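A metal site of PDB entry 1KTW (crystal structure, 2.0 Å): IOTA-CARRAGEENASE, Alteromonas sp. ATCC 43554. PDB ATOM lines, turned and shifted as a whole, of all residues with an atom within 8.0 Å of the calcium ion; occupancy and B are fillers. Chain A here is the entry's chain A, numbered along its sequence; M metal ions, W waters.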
ATOM      1  N   GLY A  29      -2.309  -2.239  13.794  1.00  0.00           N
ATOM      2  CA  GLY A  29      -1.527  -1.676  12.701  1.00  0.00           C
ATOM      3  C   GLY A  29      -2.135  -1.284  11.362  1.00  0.00           C
ATOM      4  O   GLY A  29      -1.406  -1.180  10.362  1.00  0.00           O
ATOM      5  N   ALA A  30      -3.452  -1.078  11.301  1.00  0.00           N
ATOM      6  CA  ALA A  30      -4.057  -0.658  10.036  1.00  0.00           C
ATOM      7  C   ALA A  30      -3.558   0.776   9.741  1.00  0.00           C
ATOM      8  O   ALA A  30      -3.117   1.460  10.645  1.00  0.00           O
ATOM      9  CB  ALA A  30      -5.596  -0.659  10.162  1.00  0.00           C
ATOM     10  N   ASN A  31      -3.624   1.210   8.485  1.00  0.00           N
ATOM     11  CA  ASN A  31      -3.176   2.567   8.125  1.00  0.00           C
ATOM     12  C   ASN A  31      -4.317   3.315   7.418  1.00  0.00           C
ATOM     13  O   ASN A  31      -4.684   2.957   6.309  1.00  0.00           O
ATOM     14  CB  ASN A  31      -1.952   2.489   7.200  1.00  0.00           C
ATOM     15  CG  ASN A  31      -1.305   3.846   6.947  1.00  0.00           C
ATOM     16  OD1 ASN A  31      -1.977   4.884   6.898  1.00  0.00           O
ATOM     17  ND2 ASN A  31       0.013   3.847   6.769  1.00  0.00           N
ATOM     18  N   GLY A  32      -4.858   4.348   8.060  1.00  0.00           N
ATOM     19  CA  GLY A  32      -5.952   5.116   7.482  1.00  0.00           C
ATOM     20  C   GLY A  32      -5.526   6.349   6.709  1.00  0.00           C
ATOM     21  O   GLY A  32      -6.349   7.211   6.392  1.00  0.00           O
ATOM     22  N   ASN A  33      -4.238   6.436   6.393  1.00  0.00           N
ATOM     23  CA  ASN A  33      -3.702   7.578   5.660  1.00  0.00           C
ATOM     24  C   ASN A  33      -3.132   7.207   4.293  1.00  0.00           C
ATOM     25  O   ASN A  33      -2.494   8.034   3.643  1.00  0.00           O
ATOM     26  CB  ASN A  33      -2.609   8.278   6.492  1.00  0.00           C
ATOM     27  CG  ASN A  33      -3.117   8.808   7.828  1.00  0.00           C
ATOM     28  OD1 ASN A  33      -2.505   8.583   8.878  1.00  0.00           O
ATOM     29  ND2 ASN A  33      -4.239   9.529   7.806  1.00  0.00           N
ATOM     30  N   ASP A  34      -3.350   5.964   3.857  1.00  0.00           N
ATOM     31  CA  ASP A  34      -2.833   5.530   2.559  1.00  0.00           C
ATOM     32  C   ASP A  34      -3.922   4.927   1.679  1.00  0.00           C
ATOM     33  O   ASP A  34      -5.111   5.008   2.012  1.00  0.00           O
ATOM     34  CB  ASP A  34      -1.679   4.516   2.735  1.00  0.00           C
ATOM     35  CG  ASP A  34      -2.130   3.200   3.337  1.00  0.00           C
ATOM     36  OD1 ASP A  34      -3.361   2.966   3.406  1.00  0.00           O
ATOM     37  OD2 ASP A  34      -1.267   2.394   3.738  1.00  0.00           O
ATOM     38  N   THR A  35      -3.526   4.331   0.557  1.00  0.00           N
ATOM     39  CA  THR A  35      -4.502   3.731  -0.341  1.00  0.00           C
ATOM     40  C   THR A  35      -4.411   2.198  -0.371  1.00  0.00           C
ATOM     41  O   THR A  35      -4.975   1.574  -1.260  1.00  0.00           O
ATOM     42  CB  THR A  35      -4.351   4.271  -1.809  1.00  0.00           C
ATOM     43  OG1 THR A  35      -3.062   3.902  -2.326  1.00  0.00           O
ATOM     44  CG2 THR A  35      -4.478   5.779  -1.842  1.00  0.00           C
ATOM     45  N   SER A  36      -3.729   1.616   0.619  1.00  0.00           N
ATOM     46  CA  SER A  36      -3.528   0.159   0.682  1.00  0.00           C
ATOM     47  C   SER A  36      -4.532  -0.642   1.535  1.00  0.00           C
ATOM     48  O   SER A  36      -5.170  -0.101   2.445  1.00  0.00           O
ATOM     49  CB  SER A  36      -2.117  -0.165   1.192  1.00  0.00           C
ATOM     50  OG  SER A  36      -1.132   0.294   0.288  1.00  0.00           O
ATOM     51  N   ASP A  37      -4.625  -1.938   1.231  1.00  0.00           N
ATOM     52  CA  ASP A  37      -5.532  -2.882   1.897  1.00  0.00           C
ATOM     53  C   ASP A  37      -5.312  -3.017   3.416  1.00  0.00           C
ATOM     54  O   ASP A  37      -4.173  -3.138   3.894  1.00  0.00           O
ATOM     55  CB  ASP A  37      -5.402  -4.254   1.214  1.00  0.00           C
ATOM     56  CG  ASP A  37      -6.397  -5.287   1.758  1.00  0.00           C
ATOM     57  OD1 ASP A  37      -7.615  -4.979   1.844  1.00  0.00           O
ATOM     58  OD2 ASP A  37      -5.980  -6.416   2.070  1.00  0.00           O
ATOM     59  N   ASP A  38      -6.420  -3.006   4.157  1.00  0.00           N
ATOM     60  CA  ASP A  38      -6.409  -3.114   5.623  1.00  0.00           C
ATOM     61  C   ASP A  38      -7.163  -4.371   6.111  1.00  0.00           C
ATOM     62  O   ASP A  38      -7.430  -4.522   7.308  1.00  0.00           O
ATOM     63  CB  ASP A  38      -7.091  -1.858   6.219  1.00  0.00           C
ATOM     64  CG  ASP A  38      -6.403  -0.558   5.793  1.00  0.00           C
ATOM     65  OD1 ASP A  38      -5.252  -0.328   6.233  1.00  0.00           O
ATOM     66  OD2 ASP A  38      -6.998   0.232   5.009  1.00  0.00           O
ATOM     67  N   SER A  39      -7.498  -5.271   5.186  1.00  0.00           N
ATOM     68  CA  SER A  39      -8.248  -6.487   5.530  1.00  0.00           C
ATOM     69  C   SER A  39      -7.581  -7.415   6.546  1.00  0.00           C
ATOM     70  O   SER A  39      -8.258  -7.964   7.413  1.00  0.00           O
ATOM     71  CB  SER A  39      -8.592  -7.278   4.264  1.00  0.00           C
ATOM     72  OG  SER A  39      -9.330  -6.478   3.344  1.00  0.00           O
ATOM     73  N   THR A  64      -9.199   6.827   6.101  1.00  0.00           N
ATOM     74  CA  THR A  64      -9.750   6.138   4.925  1.00  0.00           C
ATOM     75  C   THR A  64      -9.186   4.698   4.910  1.00  0.00           C
ATOM     76  O   THR A  64      -7.960   4.513   4.968  1.00  0.00           O
ATOM     77  CB  THR A  64      -9.348   6.865   3.587  1.00  0.00           C
ATOM     78  OG1 THR A  64      -9.938   8.180   3.534  1.00  0.00           O
ATOM     79  CG2 THR A  64      -9.818   6.068   2.373  1.00  0.00           C
ATOM     80  N   TYR A  65     -10.061   3.689   4.838  1.00  0.00           N
ATOM     81  CA  TYR A  65      -9.655   2.286   4.838  1.00  0.00           C
ATOM     82  C   TYR A  65     -10.182   1.505   3.631  1.00  0.00           C
ATOM     83  O   TYR A  65     -11.219   1.856   3.059  1.00  0.00           O
ATOM     84  CB  TYR A  65     -10.145   1.574   6.122  1.00  0.00           C
ATOM     85  CG  TYR A  65      -9.747   2.269   7.410  1.00  0.00           C
ATOM     86  CD1 TYR A  65      -8.557   1.946   8.060  1.00  0.00           C
ATOM     87  CD2 TYR A  65     -10.531   3.304   7.936  1.00  0.00           C
ATOM     88  CE1 TYR A  65      -8.144   2.651   9.205  1.00  0.00           C
ATOM     89  CE2 TYR A  65     -10.132   4.011   9.070  1.00  0.00           C
ATOM     90  CZ  TYR A  65      -8.934   3.684   9.699  1.00  0.00           C
ATOM     91  OH  TYR A  65      -8.511   4.428  10.786  1.00  0.00           O
ATOM     92  N   HIS A  66      -9.461   0.428   3.275  1.00  0.00           N
ATOM     93  CA  HIS A  66      -9.828  -0.470   2.170  1.00  0.00           C
ATOM     94  C   HIS A  66     -10.048  -1.913   2.711  1.00  0.00           C
ATOM     95  O   HIS A  66      -9.140  -2.484   3.309  1.00  0.00           O
ATOM     96  CB  HIS A  66      -8.710  -0.464   1.090  1.00  0.00           C
ATOM     97  CG  HIS A  66      -8.672   0.802   0.282  1.00  0.00           C
ATOM     98  ND1 HIS A  66      -8.176   1.997   0.764  1.00  0.00           N
ATOM     99  CD2 HIS A  66      -9.090   1.066  -0.986  1.00  0.00           C
ATOM    100  CE1 HIS A  66      -8.300   2.937  -0.156  1.00  0.00           C
ATOM    101  NE2 HIS A  66      -8.857   2.397  -1.228  1.00  0.00           N
ATOM    102  N   PHE A  67     -11.244  -2.487   2.490  1.00  0.00           N
ATOM    103  CA  PHE A  67     -11.567  -3.850   2.953  1.00  0.00           C
ATOM    104  C   PHE A  67     -12.308  -4.680   1.895  1.00  0.00           C
ATOM    105  O   PHE A  67     -12.956  -4.120   0.997  1.00  0.00           O
ATOM    106  CB  PHE A  67     -12.535  -3.854   4.164  1.00  0.00           C
ATOM    107  CG  PHE A  67     -12.074  -3.060   5.379  1.00  0.00           C
ATOM    108  CD1 PHE A  67     -10.851  -3.333   6.008  1.00  0.00           C
ATOM    109  CD2 PHE A  67     -12.912  -2.082   5.929  1.00  0.00           C
ATOM    110  CE1 PHE A  67     -10.481  -2.648   7.173  1.00  0.00           C
ATOM    111  CE2 PHE A  67     -12.536  -1.389   7.081  1.00  0.00           C
ATOM    112  CZ  PHE A  67     -11.319  -1.676   7.704  1.00  0.00           C
ATOM    113  N   THR A  89     -11.509  -3.020  -1.419  1.00  0.00           N
ATOM    114  CA  THR A  89     -10.173  -3.351  -1.910  1.00  0.00           C
ATOM    115  C   THR A  89     -10.355  -4.008  -3.289  1.00  0.00           C
ATOM    116  O   THR A  89     -11.227  -4.851  -3.467  1.00  0.00           O
ATOM    117  CB  THR A  89      -9.461  -4.370  -0.980  1.00  0.00           C
ATOM    118  OG1 THR A  89      -9.348  -3.825   0.349  1.00  0.00           O
ATOM    119  CG2 THR A  89      -8.042  -4.719  -1.512  1.00  0.00           C
HETATM  120 CA    CA M   1      -4.882   1.374   4.385  1.00  0.00          CA
HETATM  121  O   HOH W   1      -6.349   2.996   3.500  1.00  0.00           O
HETATM  122  O   HOH W   2      -2.724   0.175   4.631  1.00  0.00           O
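The backbone carbonyl oxygen of His 66 lies within hydrogen-bond range of the backbone NH of Asp 38. OD1 of Asn 31 lies within hydrogen-bond range of N of Asn 33 (2.8 Å).
Water W1 lies within hydrogen-bond range of O of Thr 64 (2.7 Å), O of Asp 34 (2.8 Å) and ND1 of His 66 (3.4 Å).
The calcium ion is bound by water W1 (2.4 Å), the side-chain carboxylate (OD1) of Asp 34 (2.4 Å), the backbone carbonyl oxygen (O) of Ser 36 (2.5 Å), water W2 (2.5 Å), the side-chain carboxylate (OD2) of Asp 38 (2.5 Å), the backbone carbonyl oxygen (O) of Asn 31 (2.5 Å) and the side-chain carboxylate (OD1) of Asp 38 (2.5 Å).
Of the 16 residues printed, 4 come within 4 Å of the calcium ion. Along chain A the residues within 4 Å of the calcium ion span positions 31 to 38.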
